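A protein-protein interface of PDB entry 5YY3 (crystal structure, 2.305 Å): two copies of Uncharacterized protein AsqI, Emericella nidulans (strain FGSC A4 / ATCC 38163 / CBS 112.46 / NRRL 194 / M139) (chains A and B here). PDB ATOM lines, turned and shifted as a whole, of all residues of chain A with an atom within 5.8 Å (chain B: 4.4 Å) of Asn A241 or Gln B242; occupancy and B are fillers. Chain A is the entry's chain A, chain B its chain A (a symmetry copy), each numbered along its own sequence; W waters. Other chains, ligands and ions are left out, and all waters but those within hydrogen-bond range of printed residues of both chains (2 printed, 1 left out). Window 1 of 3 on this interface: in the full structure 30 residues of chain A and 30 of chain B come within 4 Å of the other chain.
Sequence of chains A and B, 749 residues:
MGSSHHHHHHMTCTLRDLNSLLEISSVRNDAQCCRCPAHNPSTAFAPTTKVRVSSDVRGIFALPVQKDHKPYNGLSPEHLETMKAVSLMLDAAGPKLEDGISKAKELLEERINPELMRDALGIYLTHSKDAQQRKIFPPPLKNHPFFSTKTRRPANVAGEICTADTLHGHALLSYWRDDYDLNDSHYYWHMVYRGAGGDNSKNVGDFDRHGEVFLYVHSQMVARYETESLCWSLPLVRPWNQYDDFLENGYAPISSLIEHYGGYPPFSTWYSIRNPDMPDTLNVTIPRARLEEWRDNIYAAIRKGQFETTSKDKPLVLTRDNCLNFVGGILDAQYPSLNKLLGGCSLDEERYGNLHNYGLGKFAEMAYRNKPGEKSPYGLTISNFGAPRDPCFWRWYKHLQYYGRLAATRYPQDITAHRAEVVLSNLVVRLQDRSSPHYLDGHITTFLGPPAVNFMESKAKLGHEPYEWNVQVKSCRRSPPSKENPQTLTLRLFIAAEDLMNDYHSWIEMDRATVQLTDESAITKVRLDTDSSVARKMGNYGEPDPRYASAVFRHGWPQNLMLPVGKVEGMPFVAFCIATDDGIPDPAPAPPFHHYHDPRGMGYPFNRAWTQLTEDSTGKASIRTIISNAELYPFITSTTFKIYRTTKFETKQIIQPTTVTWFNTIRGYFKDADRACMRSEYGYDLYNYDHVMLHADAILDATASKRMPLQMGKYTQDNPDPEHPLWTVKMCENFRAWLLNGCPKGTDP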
ATOM      1  N   PRO A 239     -33.239 -16.839  -3.838  1.00  0.00           N
ATOM      2  CA  PRO A 239     -32.883 -16.766  -2.414  1.00  0.00           C
ATOM      3  C   PRO A 239     -31.660 -15.902  -2.194  1.00  0.00           C
ATOM      4  O   PRO A 239     -30.857 -15.738  -3.111  1.00  0.00           O
ATOM      5  CB  PRO A 239     -32.604 -18.221  -2.039  1.00  0.00           C
ATOM      6  CG  PRO A 239     -32.272 -18.888  -3.337  1.00  0.00           C
ATOM      7  CD  PRO A 239     -33.056 -18.186  -4.403  1.00  0.00           C
ATOM      8  N   TRP A 240     -31.535 -15.344  -0.996  1.00  0.00           N
ATOM      9  CA  TRP A 240     -30.368 -14.552  -0.626  1.00  0.00           C
ATOM     10  C   TRP A 240     -29.262 -15.473  -0.155  1.00  0.00           C
ATOM     11  O   TRP A 240     -28.832 -15.393   1.004  1.00  0.00           O
ATOM     12  CB  TRP A 240     -30.730 -13.556   0.479  1.00  0.00           C
ATOM     13  CG  TRP A 240     -29.691 -12.484   0.711  1.00  0.00           C
ATOM     14  CD1 TRP A 240     -28.738 -12.455   1.686  1.00  0.00           C
ATOM     15  CD2 TRP A 240     -29.524 -11.282  -0.048  1.00  0.00           C
ATOM     16  NE1 TRP A 240     -27.989 -11.316   1.581  1.00  0.00           N
ATOM     17  CE2 TRP A 240     -28.448 -10.575   0.523  1.00  0.00           C
ATOM     18  CE3 TRP A 240     -30.185 -10.732  -1.157  1.00  0.00           C
ATOM     19  CZ2 TRP A 240     -28.013  -9.354   0.026  1.00  0.00           C
ATOM     20  CZ3 TRP A 240     -29.753  -9.528  -1.655  1.00  0.00           C
ATOM     21  CH2 TRP A 240     -28.670  -8.846  -1.064  1.00  0.00           C
ATOM     22  N   ASN A 241     -28.835 -16.375  -1.040  1.00  0.00           N
ATOM     23  CA  ASN A 241     -27.804 -17.362  -0.707  1.00  0.00           C
ATOM     24  C   ASN A 241     -26.393 -16.798  -0.869  1.00  0.00           C
ATOM     25  O   ASN A 241     -25.477 -17.178  -0.136  1.00  0.00           O
ATOM     26  CB  ASN A 241     -27.966 -18.620  -1.563  1.00  0.00           C
ATOM     27  CG  ASN A 241     -29.126 -19.503  -1.100  1.00  0.00           C
ATOM     28  OD1 ASN A 241     -29.481 -19.512   0.077  1.00  0.00           O
ATOM     29  ND2 ASN A 241     -29.730 -20.235  -2.034  1.00  0.00           N
ATOM     30  N   GLN A 242     -26.236 -15.898  -1.841  1.00  0.00           N
ATOM     31  CA  GLN A 242     -24.996 -15.181  -2.081  1.00  0.00           C
ATOM     32  C   GLN A 242     -25.118 -13.765  -1.484  1.00  0.00           C
ATOM     33  O   GLN A 242     -25.953 -12.970  -1.908  1.00  0.00           O
ATOM     34  CB  GLN A 242     -24.685 -15.146  -3.594  1.00  0.00           C
ATOM     35  CG  GLN A 242     -24.696 -16.542  -4.275  1.00  0.00           C
ATOM     36  CD  GLN A 242     -24.368 -16.514  -5.789  1.00  0.00           C
ATOM     37  OE1 GLN A 242     -24.214 -15.444  -6.400  1.00  0.00           O
ATOM     38  NE2 GLN A 242     -24.287 -17.706  -6.400  1.00  0.00           N
ATOM     39  N   TYR A 243     -24.299 -13.454  -0.489  1.00  0.00           N
ATOM     40  CA  TYR A 243     -24.496 -12.222   0.287  1.00  0.00           C
ATOM     41  C   TYR A 243     -23.967 -10.963  -0.422  1.00  0.00           C
ATOM     42  O   TYR A 243     -24.198  -9.843   0.036  1.00  0.00           O
ATOM     43  CB  TYR A 243     -23.841 -12.345   1.677  1.00  0.00           C
ATOM     44  CG  TYR A 243     -24.433 -13.410   2.572  1.00  0.00           C
ATOM     45  CD1 TYR A 243     -25.588 -14.101   2.202  1.00  0.00           C
ATOM     46  CD2 TYR A 243     -23.823 -13.741   3.794  1.00  0.00           C
ATOM     47  CE1 TYR A 243     -26.127 -15.091   3.021  1.00  0.00           C
ATOM     48  CE2 TYR A 243     -24.355 -14.730   4.622  1.00  0.00           C
ATOM     49  CZ  TYR A 243     -25.510 -15.393   4.229  1.00  0.00           C
ATOM     50  OH  TYR A 243     -26.054 -16.366   5.035  1.00  0.00           O
ATOM     51  N   ARG A 295     -22.466 -18.651   7.966  1.00  0.00           N
ATOM     52  CA  ARG A 295     -23.205 -19.437   6.977  1.00  0.00           C
ATOM     53  C   ARG A 295     -22.421 -20.677   6.558  1.00  0.00           C
ATOM     54  O   ARG A 295     -22.969 -21.778   6.513  1.00  0.00           O
ATOM     55  CB  ARG A 295     -23.520 -18.589   5.735  1.00  0.00           C
ATOM     56  CG  ARG A 295     -24.090 -19.382   4.552  1.00  0.00           C
ATOM     57  CD  ARG A 295     -23.918 -18.615   3.245  1.00  0.00           C
ATOM     58  NE  ARG A 295     -22.514 -18.591   2.852  1.00  0.00           N
ATOM     59  CZ  ARG A 295     -21.981 -17.743   1.975  1.00  0.00           C
ATOM     60  NH1 ARG A 295     -22.740 -16.820   1.399  1.00  0.00           N
ATOM     61  NH2 ARG A 295     -20.677 -17.808   1.684  1.00  0.00           N
ATOM     62  N   TYR A 299     -23.360 -24.511   7.199  1.00  0.00           N
ATOM     63  CA  TYR A 299     -23.433 -25.428   6.060  1.00  0.00           C
ATOM     64  C   TYR A 299     -22.622 -26.692   6.346  1.00  0.00           C
ATOM     65  O   TYR A 299     -23.104 -27.825   6.186  1.00  0.00           O
ATOM     66  CB  TYR A 299     -22.907 -24.778   4.784  1.00  0.00           C
ATOM     67  CG  TYR A 299     -23.832 -23.786   4.090  1.00  0.00           C
ATOM     68  CD1 TYR A 299     -25.151 -23.609   4.492  1.00  0.00           C
ATOM     69  CD2 TYR A 299     -23.369 -23.033   3.018  1.00  0.00           C
ATOM     70  CE1 TYR A 299     -25.980 -22.692   3.845  1.00  0.00           C
ATOM     71  CE2 TYR A 299     -24.188 -22.139   2.366  1.00  0.00           C
ATOM     72  CZ  TYR A 299     -25.492 -21.970   2.778  1.00  0.00           C
ATOM     73  OH  TYR A 299     -26.281 -21.054   2.113  1.00  0.00           O
ATOM     74  N   ARG A 395     -36.497 -12.683   0.161  1.00  0.00           N
ATOM     75  CA  ARG A 395     -35.285 -13.322  -0.343  1.00  0.00           C
ATOM     76  C   ARG A 395     -34.471 -13.881   0.837  1.00  0.00           C
ATOM     77  O   ARG A 395     -33.865 -14.949   0.731  1.00  0.00           O
ATOM     78  CB  ARG A 395     -34.459 -12.349  -1.198  1.00  0.00           C
ATOM     79  CG  ARG A 395     -35.230 -11.813  -2.427  1.00  0.00           C
ATOM     80  CD  ARG A 395     -34.288 -11.198  -3.487  1.00  0.00           C
ATOM     81  NE  ARG A 395     -33.156 -12.090  -3.655  1.00  0.00           N
ATOM     82  CZ  ARG A 395     -32.025 -11.771  -4.265  1.00  0.00           C
ATOM     83  NH1 ARG A 395     -31.876 -10.561  -4.810  1.00  0.00           N
ATOM     84  NH2 ARG A 395     -31.045 -12.674  -4.325  1.00  0.00           N
ATOM     85  N   LYS A 398     -36.364 -17.047   2.090  1.00  0.00           N
ATOM     86  CA  LYS A 398     -36.103 -18.233   1.273  1.00  0.00           C
ATOM     87  C   LYS A 398     -34.688 -18.762   1.533  1.00  0.00           C
ATOM     88  O   LYS A 398     -34.446 -19.962   1.401  1.00  0.00           O
ATOM     89  CB  LYS A 398     -36.305 -17.972  -0.225  1.00  0.00           C
ATOM     90  CG  LYS A 398     -36.172 -19.266  -1.044  1.00  0.00           C
ATOM     91  CD  LYS A 398     -36.760 -19.155  -2.437  1.00  0.00           C
ATOM     92  CE  LYS A 398     -36.352 -20.346  -3.307  1.00  0.00           C
ATOM     93  NZ  LYS A 398     -36.807 -20.192  -4.738  1.00  0.00           N
ATOM     94  N   HIS A 399     -33.764 -17.882   1.931  1.00  0.00           N
ATOM     95  CA  HIS A 399     -32.440 -18.336   2.372  1.00  0.00           C
ATOM     96  C   HIS A 399     -32.548 -19.169   3.639  1.00  0.00           C
ATOM     97  O   HIS A 399     -31.964 -20.241   3.711  1.00  0.00           O
ATOM     98  CB  HIS A 399     -31.493 -17.163   2.620  1.00  0.00           C
ATOM     99  CG  HIS A 399     -30.156 -17.572   3.165  1.00  0.00           C
ATOM    100  ND1 HIS A 399     -29.335 -18.482   2.530  1.00  0.00           N
ATOM    101  CD2 HIS A 399     -29.491 -17.181   4.279  1.00  0.00           C
ATOM    102  CE1 HIS A 399     -28.227 -18.639   3.227  1.00  0.00           C
ATOM    103  NE2 HIS A 399     -28.295 -17.859   4.292  1.00  0.00           N
ATOM    104  N   GLN A 401     -35.078 -20.842   4.457  1.00  0.00           N
ATOM    105  CA  GLN A 401     -35.689 -22.094   4.008  1.00  0.00           C
ATOM    106  C   GLN A 401     -34.633 -23.076   3.479  1.00  0.00           C
ATOM    107  O   GLN A 401     -34.799 -24.301   3.584  1.00  0.00           O
ATOM    108  CB  GLN A 401     -36.738 -21.831   2.928  1.00  0.00           C
ATOM    109  CG  GLN A 401     -37.579 -23.054   2.574  1.00  0.00           C
ATOM    110  CD  GLN A 401     -38.306 -22.901   1.241  1.00  0.00           C
ATOM    111  OE1 GLN A 401     -37.678 -22.677   0.195  1.00  0.00           O
ATOM    112  NE2 GLN A 401     -39.637 -23.023   1.270  1.00  0.00           N
ATOM    113  N   TYR A 402     -33.546 -22.541   2.924  1.00  0.00           N
ATOM    114  CA  TYR A 402     -32.480 -23.381   2.366  1.00  0.00           C
ATOM    115  C   TYR A 402     -31.860 -24.282   3.440  1.00  0.00           C
ATOM    116  O   TYR A 402     -31.583 -25.463   3.193  1.00  0.00           O
ATOM    117  CB  TYR A 402     -31.404 -22.512   1.693  1.00  0.00           C
ATOM    118  CG  TYR A 402     -30.234 -23.287   1.137  1.00  0.00           C
ATOM    119  CD1 TYR A 402     -30.434 -24.387   0.318  1.00  0.00           C
ATOM    120  CD2 TYR A 402     -28.922 -22.903   1.415  1.00  0.00           C
ATOM    121  CE1 TYR A 402     -29.370 -25.113  -0.196  1.00  0.00           C
ATOM    122  CE2 TYR A 402     -27.838 -23.613   0.901  1.00  0.00           C
ATOM    123  CZ  TYR A 402     -28.069 -24.719   0.096  1.00  0.00           C
ATOM    124  OH  TYR A 402     -27.009 -25.432  -0.428  1.00  0.00           O
ATOM    125  N   ARG A 405     -34.070 -27.138   3.811  1.00  0.00           N
ATOM    126  CA  ARG A 405     -33.917 -28.113   2.732  1.00  0.00           C
ATOM    127  C   ARG A 405     -32.708 -29.022   2.950  1.00  0.00           C
ATOM    128  O   ARG A 405     -32.794 -30.235   2.722  1.00  0.00           O
ATOM    129  CB  ARG A 405     -33.794 -27.411   1.378  1.00  0.00           C
ATOM    130  CG  ARG A 405     -35.035 -26.625   0.992  1.00  0.00           C
ATOM    131  CD  ARG A 405     -34.860 -25.930  -0.355  1.00  0.00           C
ATOM    132  NE  ARG A 405     -36.093 -25.256  -0.747  1.00  0.00           N
ATOM    133  CZ  ARG A 405     -37.026 -25.825  -1.492  1.00  0.00           C
ATOM    134  NH1 ARG A 405     -36.850 -27.074  -1.907  1.00  0.00           N
ATOM    135  NH2 ARG A 405     -38.132 -25.165  -1.798  1.00  0.00           N
ATOM    136  N   TRP B 240     -27.892 -22.153 -10.140  1.00  0.00           N
ATOM    137  CA  TRP B 240     -28.298 -23.509  -9.786  1.00  0.00           C
ATOM    138  C   TRP B 240     -27.578 -23.938  -8.524  1.00  0.00           C
ATOM    139  O   TRP B 240     -26.806 -24.906  -8.543  1.00  0.00           O
ATOM    140  CB  TRP B 240     -27.976 -24.474 -10.930  1.00  0.00           C
ATOM    141  CG  TRP B 240     -28.634 -25.828 -10.801  1.00  0.00           C
ATOM    142  CD1 TRP B 240     -28.070 -26.979 -10.335  1.00  0.00           C
ATOM    143  CD2 TRP B 240     -29.980 -26.158 -11.160  1.00  0.00           C
ATOM    144  NE1 TRP B 240     -28.977 -28.002 -10.380  1.00  0.00           N
ATOM    145  CE2 TRP B 240     -30.161 -27.527 -10.882  1.00  0.00           C
ATOM    146  CE3 TRP B 240     -31.051 -25.427 -11.696  1.00  0.00           C
ATOM    147  CZ2 TRP B 240     -31.364 -28.180 -11.114  1.00  0.00           C
ATOM    148  CZ3 TRP B 240     -32.244 -26.068 -11.919  1.00  0.00           C
ATOM    149  CH2 TRP B 240     -32.396 -27.438 -11.627  1.00  0.00           C
ATOM    150  N   ASN B 241     -27.797 -23.189  -7.442  1.00  0.00           N
ATOM    151  CA  ASN B 241     -27.132 -23.457  -6.164  1.00  0.00           C
ATOM    152  C   ASN B 241     -27.857 -24.529  -5.351  1.00  0.00           C
ATOM    153  O   ASN B 241     -27.226 -25.293  -4.616  1.00  0.00           O
ATOM    154  CB  ASN B 241     -27.006 -22.173  -5.343  1.00  0.00           C
ATOM    155  CG  ASN B 241     -25.901 -21.249  -5.858  1.00  0.00           C
ATOM    156  OD1 ASN B 241     -24.918 -21.705  -6.439  1.00  0.00           O
ATOM    157  ND2 ASN B 241     -26.072 -19.943  -5.661  1.00  0.00           N
ATOM    158  N   GLN B 242     -29.183 -24.564  -5.489  1.00  0.00           N
ATOM    159  CA  GLN B 242     -30.029 -25.572  -4.876  1.00  0.00           C
ATOM    160  C   GLN B 242     -30.399 -26.624  -5.940  1.00  0.00           C
ATOM    161  O   GLN B 242     -31.056 -26.316  -6.932  1.00  0.00           O
ATOM    162  CB  GLN B 242     -31.281 -24.912  -4.255  1.00  0.00           C
ATOM    163  CG  GLN B 242     -30.964 -23.743  -3.283  1.00  0.00           C
ATOM    164  CD  GLN B 242     -32.214 -23.087  -2.645  1.00  0.00           C
ATOM    165  OE1 GLN B 242     -33.363 -23.422  -2.978  1.00  0.00           O
ATOM    166  NE2 GLN B 242     -31.983 -22.127  -1.738  1.00  0.00           N
ATOM    167  N   TYR B 243     -29.966 -27.862  -5.746  1.00  0.00           N
ATOM    168  CA  TYR B 243     -30.073 -28.869  -6.810  1.00  0.00           C
ATOM    169  C   TYR B 243     -31.480 -29.478  -6.935  1.00  0.00           C
ATOM    170  O   TYR B 243     -31.759 -30.221  -7.877  1.00  0.00           O
ATOM    171  CB  TYR B 243     -29.040 -29.994  -6.598  1.00  0.00           C
ATOM    172  CG  TYR B 243     -27.595 -29.561  -6.683  1.00  0.00           C
ATOM    173  CD1 TYR B 243     -27.252 -28.268  -7.085  1.00  0.00           C
ATOM    174  CD2 TYR B 243     -26.558 -30.447  -6.343  1.00  0.00           C
ATOM    175  CE1 TYR B 243     -25.920 -27.865  -7.150  1.00  0.00           C
ATOM    176  CE2 TYR B 243     -25.221 -30.054  -6.406  1.00  0.00           C
ATOM    177  CZ  TYR B 243     -24.914 -28.763  -6.817  1.00  0.00           C
ATOM    178  OH  TYR B 243     -23.602 -28.359  -6.894  1.00  0.00           O
ATOM    179  N   ASP B 244     -32.360 -29.167  -5.989  1.00  0.00           N
ATOM    180  CA  ASP B 244     -33.755 -29.577  -6.076  1.00  0.00           C
ATOM    181  C   ASP B 244     -34.608 -28.466  -6.672  1.00  0.00           C
ATOM    182  O   ASP B 244     -35.797 -28.349  -6.382  1.00  0.00           O
ATOM    183  CB  ASP B 244     -34.283 -29.964  -4.696  1.00  0.00           C
ATOM    184  CG  ASP B 244     -34.141 -28.834  -3.690  1.00  0.00           C
ATOM    185  OD1 ASP B 244     -33.336 -27.906  -3.953  1.00  0.00           O
ATOM    186  OD2 ASP B 244     -34.814 -28.878  -2.632  1.00  0.00           O
ATOM    187  N   ASP B 245     -33.996 -27.642  -7.508  1.00  0.00           N
ATOM    188  CA  ASP B 245     -34.691 -26.477  -8.031  1.00  0.00           C
ATOM    189  C   ASP B 245     -35.515 -26.824  -9.270  1.00  0.00           C
ATOM    190  O   ASP B 245     -35.346 -27.885  -9.892  1.00  0.00           O
ATOM    191  CB  ASP B 245     -33.696 -25.364  -8.357  1.00  0.00           C
ATOM    192  CG  ASP B 245     -34.324 -23.984  -8.328  1.00  0.00           C
ATOM    193  OD1 ASP B 245     -35.570 -23.904  -8.191  1.00  0.00           O
ATOM    194  OD2 ASP B 245     -33.572 -22.985  -8.454  1.00  0.00           O
ATOM    195  N   TYR B 402     -20.136 -19.206  -8.605  1.00  0.00           N
ATOM    196  CA  TYR B 402     -20.255 -19.066  -7.149  1.00  0.00           C
ATOM    197  C   TYR B 402     -18.992 -19.558  -6.435  1.00  0.00           C
ATOM    198  O   TYR B 402     -18.520 -18.931  -5.477  1.00  0.00           O
ATOM    199  CB  TYR B 402     -21.499 -19.810  -6.636  1.00  0.00           C
ATOM    200  CG  TYR B 402     -21.676 -19.770  -5.137  1.00  0.00           C
ATOM    201  CD1 TYR B 402     -21.610 -18.571  -4.445  1.00  0.00           C
ATOM    202  CD2 TYR B 402     -21.933 -20.934  -4.414  1.00  0.00           C
ATOM    203  CE1 TYR B 402     -21.765 -18.518  -3.067  1.00  0.00           C
ATOM    204  CE2 TYR B 402     -22.101 -20.902  -3.030  1.00  0.00           C
ATOM    205  CZ  TYR B 402     -22.015 -19.689  -2.362  1.00  0.00           C
ATOM    206  OH  TYR B 402     -22.185 -19.635  -0.993  1.00  0.00           O
HETATM  207  O   HOH W   1     -24.766 -19.964  -0.105  1.00  0.00           O
HETATM  208  O   HOH W   2     -25.649 -24.200  -2.475  1.00  0.00           O
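The guanidinium group (NH2) of Arg A395 sits at hydrogen-bond distance from the backbone carbonyl oxygen (O) of Pro A239 (3.3 Å). NH1 of Arg A295 sits at hydrogen-bond distance from O of Asn A241, 3.2 Å away. A ring nitrogen (ND1) of His A399 is in hydrogen-bond range of the side-chain amide oxygen of Asn A241 (2.7 Å). OE1 of Gln A401 is in hydrogen-bond range of NE of Arg A405 (3.2 Å).
Along chain A the printed residues that touch a printed residue of chain B span positions 239 to 405. Along chain B the printed residues that touch a printed residue of chain A span positions 241 to 402. Among the printed residues, 8 pairs touch across the chains.
Water W2 lies within hydrogen-bond range of OH of Tyr A402 (2.7 Å) and O of Asn B241 (2.9 Å). Water W1 lies within hydrogen-bond range of OH of Tyr B402 (2.7 Å), O of Asn A241 (2.9 Å) and OH of Tyr A299 (2.9 Å).
Of the printed residues of chain B, Asn A241 touches Gln B242 (3.0 Å). Of the printed residues of chain A, Asn B241 touches Gln A242 (3.0 Å). Of chain A, only Pro A239 (3.6 Å), Asn A241 (3.0 Å), Tyr A402 (3.4 Å) and Arg A405 (3.9 Å) come within 4 Å of Gln B242. Printed residues of chain A within 4 Å of Tyr B402: Gln A242 (3.4 Å) and Arg A295 (3.5 Å). The nearest residue of chain A that does not touch Gln B242 is Lys A398 (4.3 Å).
Among the printed residues, pairs that only touch across the chains: Pro A239 with Gln B242 (3.6 Å), Gln A242 with Tyr B402 (3.4 Å), Arg A295 with Tyr B402 (3.5 Å), Tyr A402 with Gln B242 (3.4 Å) and Arg A405 with Gln B242 (3.9 Å).
Asn A241 touches Gln B242, and with the chains exchanged Gln A242 touches Asn B241. Gln A242 touches Tyr B402, and with the chains exchanged Tyr A402 touches Gln B242. Of the 8 pairs that touch across the chains among the printed residues, 4 have their exchanged pair printed and touching as well.
ND2 of Asn A241 sits close to NE2 of Gln B242 (3.0 Å). The side-chain amide nitrogen (NE2) of Gln A242 lies close to the side-chain amide nitrogen (ND2) of Asn B241 (3.0 Å). The side-chain carboxylate (OD2) of Asp B244 is in salt-bridge range of the guanidinium group (NH1) of Arg A405 (2.8 Å).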
